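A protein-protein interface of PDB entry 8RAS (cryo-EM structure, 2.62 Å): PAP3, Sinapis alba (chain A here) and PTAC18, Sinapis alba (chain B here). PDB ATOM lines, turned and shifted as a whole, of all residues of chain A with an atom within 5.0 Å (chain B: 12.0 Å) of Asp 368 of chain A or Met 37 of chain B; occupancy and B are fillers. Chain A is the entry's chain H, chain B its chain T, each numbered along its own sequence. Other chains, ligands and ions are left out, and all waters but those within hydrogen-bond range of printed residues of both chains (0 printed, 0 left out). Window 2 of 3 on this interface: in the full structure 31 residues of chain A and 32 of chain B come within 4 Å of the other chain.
SD of Met 37 of chain B is in hydrogen-bond range of NH2 of Arg 335 of chain A, at 3.4 Å. The side-chain hydroxyl (OG1) of Thr 39 of chain B sits at hydrogen-bond distance from the side-chain carboxylate (OD1) of Asp 377 of chain A (2.9 Å). The side-chain hydroxyl (OH) of Tyr 45 of chain B sits at hydrogen-bond distance from the side-chain amide nitrogen (ND2) of Asn 370 of chain A (3.0 Å). The side-chain carboxylate of Glu 373 of chain A is in hydrogen-bond range of the side-chain hydroxyl of Ser 100 of chain B (3.2 Å). The side-chain carboxylate (OE1) of Glu 373 of chain A lies within salt-bridge range of the guanidinium group (NH2) of Arg 102 of chain B. The side-chain carboxylate of Asp 368 of chain A sits close to the side-chain sulfur of Met 37 of chain B (3.5 Å).
O of Arg 102 of chain B lies within hydrogen-bond range of OG of Ser 100 of chain B, 2.8 Å away. The backbone carbonyl oxygen (O) of Arg 335 of chain A lies within hydrogen-bond range of the backbone NH (N) of Phe 363 of chain A, at 2.8 Å. The side-chain carboxylate (OD2) of Asp 368 of chain A is in salt-bridge range of the guanidinium group (NH1) of Arg 335 of chain A (2.8 Å). NE of Arg 335 of chain A is in salt-bridge range of OD2 of Asp 377 of chain A, 2.8 Å away. The backbone NH (N) of Arg 365 of chain A is in hydrogen-bond range of the side-chain carboxylate (OD2) of Asp 368 of chain A. ND2 of Asn 370 of chain A lies close to OE2 of Glu 373 of chain A (3.4 Å).
Among the printed residues, merely in contact across the chains: Glu 373 of chain A with Tyr 45 of chain B (3.3 Å), Asn 370 of chain A with Gly 99 of chain B (3.5 Å), Glu 373 of chain A with Met 37 of chain B (3.5 Å), Asn 370 of chain A with Ser 100 of chain B (3.6 Å), Asp 377 of chain A with Leu 44 of chain B (3.6 Å), Asp 377 of chain A with Met 37 of chain B (3.6 Å), Thr 369 of chain A with Lys 101 of chain B (3.7 Å) and Asn 370 of chain A with Glu 98 of chain B (3.9 Å).
Arg 335 of chain A touches one residue of chain B. Arg 365 of chain A touches none of the printed residues of chain B. No residue of chain B comes within 4 Å of Asp 366 of chain A. No residue of chain B comes within 4 Å of Gly 367 of chain A. Of chain B, only Met 37 (3.5 Å) comes within 4 Å of Asp 368 of chain A. Of the printed residues of chain B, Asn 370 of chain A touches Tyr 45 (3.0 Å), Glu 98 (3.9 Å), Gly 99 (3.5 Å) and Ser 100 (3.6 Å). No residue of chain B comes within 4 Å of Ile 374 of chain A. Asp 377 of chain A touches just these residues of chain B: Met 37 (3.6 Å), Thr 39 (2.9 Å) and Leu 44 (3.6 Å). Printed residues of chain A within 4 Å of Leu 44 of chain B: Asp 377. Of the printed residues of chain A, Tyr 45 of chain B touches Asn 370 (3.0 Å) and Glu 373 (3.3 Å). Of the printed residues of chain A, Glu 98 of chain B touches Asn 370. Of the printed residues of chain A, Ser 100 of chain B touches Asn 370 and Glu 373. Met 104 of chain B touches none of the printed residues of chain A. The nearest residue of chain B that does not touch Asp 368 of chain A is Gln 38 of chain B (6.5 Å). The nearest residue of chain A that does not touch Met 37 of chain B is Gly 367 of chain A (4.2 Å).
Of the 18 printed residues of chain B, 9 touch a printed residue of chain A. Hydrophobic or aromatic side chains of chain B within 4 Å of the printed part of chain A: Met 37, Leu 44 and Tyr 45. Among the printed residues, Asp or Glu carboxylates within 4 Å of a Lys or Arg side-chain nitrogen of the other chain: Glu 373 of chain A with Arg 102 of chain B.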
ATOM      1  N   ARG A 335      28.894   9.285  -7.078  1.00  0.00           N
ATOM      2  CA  ARG A 335      27.543   8.901  -7.465  1.00  0.00           C
ATOM      3  C   ARG A 335      27.521   8.111  -8.770  1.00  0.00           C
ATOM      4  O   ARG A 335      26.850   7.080  -8.859  1.00  0.00           O
ATOM      5  CB  ARG A 335      26.661  10.149  -7.584  1.00  0.00           C
ATOM      6  CG  ARG A 335      25.289   9.900  -8.194  1.00  0.00           C
ATOM      7  CD  ARG A 335      24.453   8.963  -7.340  1.00  0.00           C
ATOM      8  NE  ARG A 335      24.473   9.337  -5.932  1.00  0.00           N
ATOM      9  CZ  ARG A 335      24.319   8.484  -4.929  1.00  0.00           C
ATOM     10  NH1 ARG A 335      24.132   7.192  -5.143  1.00  0.00           N
ATOM     11  NH2 ARG A 335      24.357   8.938  -3.681  1.00  0.00           N
ATOM     12  N   PHE A 363      26.004   4.429  -8.693  1.00  0.00           N
ATOM     13  CA  PHE A 363      26.215   3.516  -7.582  1.00  0.00           C
ATOM     14  C   PHE A 363      25.044   3.584  -6.614  1.00  0.00           C
ATOM     15  O   PHE A 363      24.361   4.605  -6.503  1.00  0.00           O
ATOM     16  CB  PHE A 363      27.505   3.851  -6.832  1.00  0.00           C
ATOM     17  CG  PHE A 363      28.755   3.424  -7.537  1.00  0.00           C
ATOM     18  CD1 PHE A 363      29.134   2.095  -7.559  1.00  0.00           C
ATOM     19  CD2 PHE A 363      29.565   4.356  -8.159  1.00  0.00           C
ATOM     20  CE1 PHE A 363      30.288   1.703  -8.201  1.00  0.00           C
ATOM     21  CE2 PHE A 363      30.719   3.969  -8.799  1.00  0.00           C
ATOM     22  CZ  PHE A 363      31.082   2.641  -8.821  1.00  0.00           C
ATOM     23  N   HIS A 364      24.820   2.484  -5.906  1.00  0.00           N
ATOM     24  CA  HIS A 364      23.848   2.423  -4.817  1.00  0.00           C
ATOM     25  C   HIS A 364      24.637   2.139  -3.542  1.00  0.00           C
ATOM     26  O   HIS A 364      24.892   0.987  -3.192  1.00  0.00           O
ATOM     27  CB  HIS A 364      22.782   1.368  -5.082  1.00  0.00           C
ATOM     28  CG  HIS A 364      21.849   1.722  -6.195  1.00  0.00           C
ATOM     29  ND1 HIS A 364      20.647   2.362  -5.984  1.00  0.00           N
ATOM     30  CD2 HIS A 364      21.942   1.530  -7.532  1.00  0.00           C
ATOM     31  CE1 HIS A 364      20.039   2.546  -7.142  1.00  0.00           C
ATOM     32  NE2 HIS A 364      20.804   2.049  -8.098  1.00  0.00           N
ATOM     33  N   ARG A 365      25.023   3.208  -2.850  1.00  0.00           N
ATOM     34  CA  ARG A 365      25.898   3.106  -1.695  1.00  0.00           C
ATOM     35  C   ARG A 365      25.121   2.647  -0.463  1.00  0.00           C
ATOM     36  O   ARG A 365      23.889   2.596  -0.447  1.00  0.00           O
ATOM     37  CB  ARG A 365      26.577   4.447  -1.423  1.00  0.00           C
ATOM     38  CG  ARG A 365      27.266   5.055  -2.632  1.00  0.00           C
ATOM     39  CD  ARG A 365      28.313   4.119  -3.198  1.00  0.00           C
ATOM     40  NE  ARG A 365      29.197   4.794  -4.140  1.00  0.00           N
ATOM     41  CZ  ARG A 365      30.520   4.785  -4.064  1.00  0.00           C
ATOM     42  NH1 ARG A 365      31.151   4.141  -3.099  1.00  0.00           N
ATOM     43  NH2 ARG A 365      31.226   5.436  -4.983  1.00  0.00           N
ATOM     44  N   ASP A 366      25.873   2.306   0.589  1.00  0.00           N
ATOM     45  CA  ASP A 366      25.254   1.880   1.839  1.00  0.00           C
ATOM     46  C   ASP A 366      24.529   3.027   2.530  1.00  0.00           C
ATOM     47  O   ASP A 366      23.533   2.799   3.226  1.00  0.00           O
ATOM     48  CB  ASP A 366      26.308   1.282   2.769  1.00  0.00           C
ATOM     49  CG  ASP A 366      27.279   2.320   3.292  1.00  0.00           C
ATOM     50  OD1 ASP A 366      27.693   3.197   2.505  1.00  0.00           O
ATOM     51  OD2 ASP A 366      27.626   2.262   4.491  1.00  0.00           O
ATOM     52  N   GLY A 367      25.010   4.258   2.359  1.00  0.00           N
ATOM     53  CA  GLY A 367      24.356   5.406   2.954  1.00  0.00           C
ATOM     54  C   GLY A 367      23.110   5.872   2.239  1.00  0.00           C
ATOM     55  O   GLY A 367      22.426   6.772   2.735  1.00  0.00           O
ATOM     56  N   ASP A 368      22.800   5.284   1.087  1.00  0.00           N
ATOM     57  CA  ASP A 368      21.617   5.653   0.315  1.00  0.00           C
ATOM     58  C   ASP A 368      20.423   4.880   0.857  1.00  0.00           C
ATOM     59  O   ASP A 368      20.198   3.724   0.494  1.00  0.00           O
ATOM     60  CB  ASP A 368      21.834   5.367  -1.166  1.00  0.00           C
ATOM     61  CG  ASP A 368      23.072   6.046  -1.715  1.00  0.00           C
ATOM     62  OD1 ASP A 368      23.630   6.919  -1.019  1.00  0.00           O
ATOM     63  OD2 ASP A 368      23.486   5.706  -2.842  1.00  0.00           O
ATOM     64  N   THR A 369      19.651   5.519   1.737  1.00  0.00           N
ATOM     65  CA  THR A 369      18.462   4.909   2.311  1.00  0.00           C
ATOM     66  C   THR A 369      17.165   5.524   1.806  1.00  0.00           C
ATOM     67  O   THR A 369      16.095   4.952   2.044  1.00  0.00           O
ATOM     68  CB  THR A 369      18.497   5.003   3.843  1.00  0.00           C
ATOM     69  OG1 THR A 369      18.229   6.351   4.250  1.00  0.00           O
ATOM     70  CG2 THR A 369      19.860   4.579   4.372  1.00  0.00           C
ATOM     71  N   ASN A 370      17.226   6.664   1.123  1.00  0.00           N
ATOM     72  CA  ASN A 370      16.044   7.321   0.581  1.00  0.00           C
ATOM     73  C   ASN A 370      16.116   7.313  -0.939  1.00  0.00           C
ATOM     74  O   ASN A 370      17.044   7.911  -1.511  1.00  0.00           O
ATOM     75  CB  ASN A 370      15.929   8.754   1.106  1.00  0.00           C
ATOM     76  CG  ASN A 370      14.649   9.436   0.668  1.00  0.00           C
ATOM     77  OD1 ASN A 370      13.717   8.787   0.193  1.00  0.00           O
ATOM     78  ND2 ASN A 370      14.596  10.753   0.826  1.00  0.00           N
ATOM     79  N   GLU A 373      16.322  10.891  -2.422  1.00  0.00           N
ATOM     80  CA  GLU A 373      17.645  11.504  -2.350  1.00  0.00           C
ATOM     81  C   GLU A 373      18.557  10.967  -3.444  1.00  0.00           C
ATOM     82  O   GLU A 373      19.339  11.720  -4.037  1.00  0.00           O
ATOM     83  CB  GLU A 373      18.262  11.266  -0.973  1.00  0.00           C
ATOM     84  CG  GLU A 373      17.599  12.043   0.149  1.00  0.00           C
ATOM     85  CD  GLU A 373      18.198  11.727   1.505  1.00  0.00           C
ATOM     86  OE1 GLU A 373      19.438  11.602   1.594  1.00  0.00           O
ATOM     87  OE2 GLU A 373      17.428  11.600   2.480  1.00  0.00           O
ATOM     88  N   ILE A 374      18.472   9.664  -3.723  1.00  0.00           N
ATOM     89  CA  ILE A 374      19.280   9.077  -4.788  1.00  0.00           C
ATOM     90  C   ILE A 374      18.903   9.684  -6.134  1.00  0.00           C
ATOM     91  O   ILE A 374      19.768  10.126  -6.898  1.00  0.00           O
ATOM     92  CB  ILE A 374      19.121   7.546  -4.803  1.00  0.00           C
ATOM     93  CG1 ILE A 374      19.514   6.950  -3.453  1.00  0.00           C
ATOM     94  CG2 ILE A 374      19.957   6.936  -5.915  1.00  0.00           C
ATOM     95  CD1 ILE A 374      18.844   5.626  -3.161  1.00  0.00           C
ATOM     96  N   ASP A 377      20.237  13.152  -6.408  1.00  0.00           N
ATOM     97  CA  ASP A 377      21.682  13.266  -6.585  1.00  0.00           C
ATOM     98  C   ASP A 377      22.063  13.141  -8.054  1.00  0.00           C
ATOM     99  O   ASP A 377      22.973  13.832  -8.528  1.00  0.00           O
ATOM    100  CB  ASP A 377      22.403  12.215  -5.744  1.00  0.00           C
ATOM    101  CG  ASP A 377      23.734  12.709  -5.214  1.00  0.00           C
ATOM    102  OD1 ASP A 377      23.993  13.928  -5.303  1.00  0.00           O
ATOM    103  OD2 ASP A 377      24.521  11.883  -4.708  1.00  0.00           O
ATOM    104  N   MET B  37      24.117  10.898   2.751  1.00  0.00           N
ATOM    105  CA  MET B  37      24.876  11.051   1.515  1.00  0.00           C
ATOM    106  C   MET B  37      25.814  12.250   1.591  1.00  0.00           C
ATOM    107  O   MET B  37      25.763  13.030   2.542  1.00  0.00           O
ATOM    108  CB  MET B  37      23.932  11.196   0.320  1.00  0.00           C
ATOM    109  CG  MET B  37      22.830  10.149   0.272  1.00  0.00           C
ATOM    110  SD  MET B  37      22.073  10.000  -1.356  1.00  0.00           S
ATOM    111  CE  MET B  37      22.171  11.691  -1.938  1.00  0.00           C
ATOM    112  N   GLN B  38      26.679  12.387   0.584  1.00  0.00           N
ATOM    113  CA  GLN B  38      27.610  13.509   0.556  1.00  0.00           C
ATOM    114  C   GLN B  38      26.881  14.832   0.354  1.00  0.00           C
ATOM    115  O   GLN B  38      27.215  15.836   0.994  1.00  0.00           O
ATOM    116  CB  GLN B  38      28.652  13.300  -0.542  1.00  0.00           C
ATOM    117  CG  GLN B  38      29.290  11.923  -0.540  1.00  0.00           C
ATOM    118  CD  GLN B  38      30.579  11.881   0.254  1.00  0.00           C
ATOM    119  OE1 GLN B  38      31.670  11.875  -0.314  1.00  0.00           O
ATOM    120  NE2 GLN B  38      30.459  11.849   1.577  1.00  0.00           N
ATOM    121  N   THR B  39      25.890  14.853  -0.527  1.00  0.00           N
ATOM    122  CA  THR B  39      25.184  16.091  -0.835  1.00  0.00           C
ATOM    123  C   THR B  39      24.214  16.437   0.289  1.00  0.00           C
ATOM    124  O   THR B  39      23.399  15.595   0.678  1.00  0.00           O
ATOM    125  CB  THR B  39      24.426  15.967  -2.153  1.00  0.00           C
ATOM    126  OG1 THR B  39      25.262  15.334  -3.130  1.00  0.00           O
ATOM    127  CG2 THR B  39      24.017  17.343  -2.660  1.00  0.00           C
ATOM    128  N   PRO B  40      24.275  17.649   0.834  1.00  0.00           N
ATOM    129  CA  PRO B  40      23.317  18.043   1.872  1.00  0.00           C
ATOM    130  C   PRO B  40      21.905  18.143   1.317  1.00  0.00           C
ATOM    131  O   PRO B  40      21.682  18.297   0.114  1.00  0.00           O
ATOM    132  CB  PRO B  40      23.833  19.410   2.336  1.00  0.00           C
ATOM    133  CG  PRO B  40      25.250  19.480   1.854  1.00  0.00           C
ATOM    134  CD  PRO B  40      25.280  18.694   0.586  1.00  0.00           C
ATOM    135  N   LEU B  41      20.936  18.044   2.232  1.00  0.00           N
ATOM    136  CA  LEU B  41      19.532  17.987   1.835  1.00  0.00           C
ATOM    137  C   LEU B  41      19.085  19.256   1.120  1.00  0.00           C
ATOM    138  O   LEU B  41      18.236  19.192   0.223  1.00  0.00           O
ATOM    139  CB  LEU B  41      18.651  17.738   3.059  1.00  0.00           C
ATOM    140  CG  LEU B  41      18.572  16.302   3.578  1.00  0.00           C
ATOM    141  CD1 LEU B  41      19.681  16.043   4.583  1.00  0.00           C
ATOM    142  CD2 LEU B  41      17.212  16.026   4.196  1.00  0.00           C
ATOM    143  N   GLU B  42      19.624  20.415   1.508  1.00  0.00           N
ATOM    144  CA  GLU B  42      19.185  21.670   0.904  1.00  0.00           C
ATOM    145  C   GLU B  42      19.491  21.705  -0.588  1.00  0.00           C
ATOM    146  O   GLU B  42      18.654  22.135  -1.391  1.00  0.00           O
ATOM    147  CB  GLU B  42      19.843  22.855   1.612  1.00  0.00           C
ATOM    148  CG  GLU B  42      19.861  22.749   3.127  1.00  0.00           C
ATOM    149  CD  GLU B  42      21.141  22.130   3.650  1.00  0.00           C
ATOM    150  OE1 GLU B  42      22.144  22.121   2.906  1.00  0.00           O
ATOM    151  OE2 GLU B  42      21.145  21.653   4.804  1.00  0.00           O
ATOM    152  N   GLU B  43      20.688  21.261  -0.978  1.00  0.00           N
ATOM    153  CA  GLU B  43      21.038  21.228  -2.394  1.00  0.00           C
ATOM    154  C   GLU B  43      20.171  20.234  -3.155  1.00  0.00           C
ATOM    155  O   GLU B  43      19.714  20.524  -4.267  1.00  0.00           O
ATOM    156  CB  GLU B  43      22.521  20.889  -2.565  1.00  0.00           C
ATOM    157  CG  GLU B  43      23.494  21.995  -2.160  1.00  0.00           C
ATOM    158  CD  GLU B  43      23.431  22.349  -0.684  1.00  0.00           C
ATOM    159  OE1 GLU B  43      22.958  21.514   0.113  1.00  0.00           O
ATOM    160  OE2 GLU B  43      23.852  23.467  -0.323  1.00  0.00           O
ATOM    161  N   LEU B  44      19.936  19.055  -2.576  1.00  0.00           N
ATOM    162  CA  LEU B  44      19.151  18.033  -3.261  1.00  0.00           C
ATOM    163  C   LEU B  44      17.708  18.477  -3.464  1.00  0.00           C
ATOM    164  O   LEU B  44      17.137  18.276  -4.542  1.00  0.00           O
ATOM    165  CB  LEU B  44      19.197  16.722  -2.479  1.00  0.00           C
ATOM    166  CG  LEU B  44      20.562  16.049  -2.332  1.00  0.00           C
ATOM    167  CD1 LEU B  44      20.545  15.051  -1.188  1.00  0.00           C
ATOM    168  CD2 LEU B  44      20.962  15.372  -3.629  1.00  0.00           C
ATOM    169  N   TYR B  45      17.103  19.081  -2.445  1.00  0.00           N
ATOM    170  CA  TYR B  45      15.690  19.427  -2.475  1.00  0.00           C
ATOM    171  C   TYR B  45      15.433  20.869  -2.887  1.00  0.00           C
ATOM    172  O   TYR B  45      14.276  21.301  -2.878  1.00  0.00           O
ATOM    173  CB  TYR B  45      15.060  19.153  -1.107  1.00  0.00           C
ATOM    174  CG  TYR B  45      14.956  17.681  -0.783  1.00  0.00           C
ATOM    175  CD1 TYR B  45      13.866  16.934  -1.206  1.00  0.00           C
ATOM    176  CD2 TYR B  45      15.952  17.036  -0.066  1.00  0.00           C
ATOM    177  CE1 TYR B  45      13.769  15.588  -0.918  1.00  0.00           C
ATOM    178  CE2 TYR B  45      15.864  15.690   0.227  1.00  0.00           C
ATOM    179  CZ  TYR B  45      14.769  14.972  -0.202  1.00  0.00           C
ATOM    180  OH  TYR B  45      14.675  13.631   0.089  1.00  0.00           O
ATOM    181  N   ASN B  46      16.477  21.618  -3.249  1.00  0.00           N
ATOM    182  CA  ASN B  46      16.348  22.986  -3.750  1.00  0.00           C
ATOM    183  C   ASN B  46      15.652  23.881  -2.721  1.00  0.00           C
ATOM    184  O   ASN B  46      14.552  24.396  -2.934  1.00  0.00           O
ATOM    185  CB  ASN B  46      15.619  23.004  -5.099  1.00  0.00           C
ATOM    186  CG  ASN B  46      15.461  24.403  -5.664  1.00  0.00           C
ATOM    187  OD1 ASN B  46      14.429  24.737  -6.245  1.00  0.00           O
ATOM    188  ND2 ASN B  46      16.487  25.229  -5.495  1.00  0.00           N
ATOM    189  N   PRO B  97      12.124  15.692   4.902  1.00  0.00           N
ATOM    190  CA  PRO B  97      11.410  15.355   3.668  1.00  0.00           C
ATOM    191  C   PRO B  97      10.880  13.929   3.707  1.00  0.00           C
ATOM    192  O   PRO B  97      11.364  13.074   4.452  1.00  0.00           O
ATOM    193  CB  PRO B  97      12.472  15.524   2.574  1.00  0.00           C
ATOM    194  CG  PRO B  97      13.586  16.303   3.219  1.00  0.00           C
ATOM    195  CD  PRO B  97      13.555  15.935   4.663  1.00  0.00           C
ATOM    196  N   GLU B  98       9.855  13.691   2.891  1.00  0.00           N
ATOM    197  CA  GLU B  98       9.184  12.396   2.865  1.00  0.00           C
ATOM    198  C   GLU B  98      10.170  11.280   2.548  1.00  0.00           C
ATOM    199  O   GLU B  98      10.752  11.240   1.459  1.00  0.00           O
ATOM    200  CB  GLU B  98       8.054  12.416   1.837  1.00  0.00           C
ATOM    201  CG  GLU B  98       7.385  11.071   1.616  1.00  0.00           C
ATOM    202  CD  GLU B  98       6.501  10.660   2.777  1.00  0.00           C
ATOM    203  OE1 GLU B  98       7.024  10.083   3.752  1.00  0.00           O
ATOM    204  OE2 GLU B  98       5.280  10.916   2.713  1.00  0.00           O
ATOM    205  N   GLY B  99      10.356  10.371   3.505  1.00  0.00           N
ATOM    206  CA  GLY B  99      11.237   9.239   3.339  1.00  0.00           C
ATOM    207  C   GLY B  99      12.671   9.468   3.762  1.00  0.00           C
ATOM    208  O   GLY B  99      13.447   8.505   3.808  1.00  0.00           O
ATOM    209  N   SER B 100      13.049  10.702   4.077  1.00  0.00           N
ATOM    210  CA  SER B 100      14.423  11.002   4.447  1.00  0.00           C
ATOM    211  C   SER B 100      14.705  10.584   5.884  1.00  0.00           C
ATOM    212  O   SER B 100      13.848  10.707   6.763  1.00  0.00           O
ATOM    213  CB  SER B 100      14.709  12.494   4.278  1.00  0.00           C
ATOM    214  OG  SER B 100      15.869  12.872   4.996  1.00  0.00           O
ATOM    215  N   LYS B 101      15.916  10.083   6.114  1.00  0.00           N
ATOM    216  CA  LYS B 101      16.385   9.756   7.453  1.00  0.00           C
ATOM    217  C   LYS B 101      17.171  10.893   8.092  1.00  0.00           C
ATOM    218  O   LYS B 101      17.652  10.737   9.218  1.00  0.00           O
ATOM    219  CB  LYS B 101      17.249   8.491   7.419  1.00  0.00           C
ATOM    220  CG  LYS B 101      16.502   7.217   7.780  1.00  0.00           C
ATOM    221  CD  LYS B 101      15.480   6.849   6.717  1.00  0.00           C
ATOM    222  CE  LYS B 101      14.442   5.884   7.264  1.00  0.00           C
ATOM    223  NZ  LYS B 101      14.877   4.466   7.137  1.00  0.00           N
ATOM    224  N   ARG B 102      17.312  12.020   7.404  1.00  0.00           N
ATOM    225  CA  ARG B 102      18.020  13.184   7.911  1.00  0.00           C
ATOM    226  C   ARG B 102      17.088  14.389   7.905  1.00  0.00           C
ATOM    227  O   ARG B 102      15.977  14.342   7.372  1.00  0.00           O
ATOM    228  CB  ARG B 102      19.278  13.469   7.081  1.00  0.00           C
ATOM    229  CG  ARG B 102      20.459  12.575   7.415  1.00  0.00           C
ATOM    230  CD  ARG B 102      21.583  12.738   6.404  1.00  0.00           C
ATOM    231  NE  ARG B 102      21.077  12.958   5.055  1.00  0.00           N
ATOM    232  CZ  ARG B 102      21.831  13.295   4.018  1.00  0.00           C
ATOM    233  NH1 ARG B 102      23.137  13.465   4.140  1.00  0.00           N
ATOM    234  NH2 ARG B 102      21.260  13.469   2.829  1.00  0.00           N
ATOM    235  N   PHE B 103      17.555  15.479   8.508  1.00  0.00           N
ATOM    236  CA  PHE B 103      16.743  16.675   8.674  1.00  0.00           C
ATOM    237  C   PHE B 103      17.558  17.907   8.312  1.00  0.00           C
ATOM    238  O   PHE B 103      18.791  17.901   8.361  1.00  0.00           O
ATOM    239  CB  PHE B 103      16.212  16.801  10.109  1.00  0.00           C
ATOM    240  CG  PHE B 103      17.289  16.778  11.158  1.00  0.00           C
ATOM    241  CD1 PHE B 103      17.917  17.947  11.553  1.00  0.00           C
ATOM    242  CD2 PHE B 103      17.671  15.587  11.749  1.00  0.00           C
ATOM    243  CE1 PHE B 103      18.908  17.927  12.514  1.00  0.00           C
ATOM    244  CE2 PHE B 103      18.660  15.561  12.713  1.00  0.00           C
ATOM    245  CZ  PHE B 103      19.278  16.733  13.096  1.00  0.00           C
ATOM    246  N   MET B 104      16.848  18.972   7.952  1.00  0.00           N
ATOM    247  CA  MET B 104      17.448  20.277   7.705  1.00  0.00           C
ATOM    248  C   MET B 104      17.219  21.153   8.929  1.00  0.00           C
ATOM    249  O   MET B 104      16.071  21.386   9.324  1.00  0.00           O
ATOM    250  CB  MET B 104      16.856  20.925   6.454  1.00  0.00           C
ATOM    251  CG  MET B 104      17.562  20.539   5.164  1.00  0.00           C
ATOM    252  SD  MET B 104      16.612  20.935   3.684  1.00  0.00           S
ATOM    253  CE  MET B 104      14.938  20.771   4.294  1.00  0.00           C
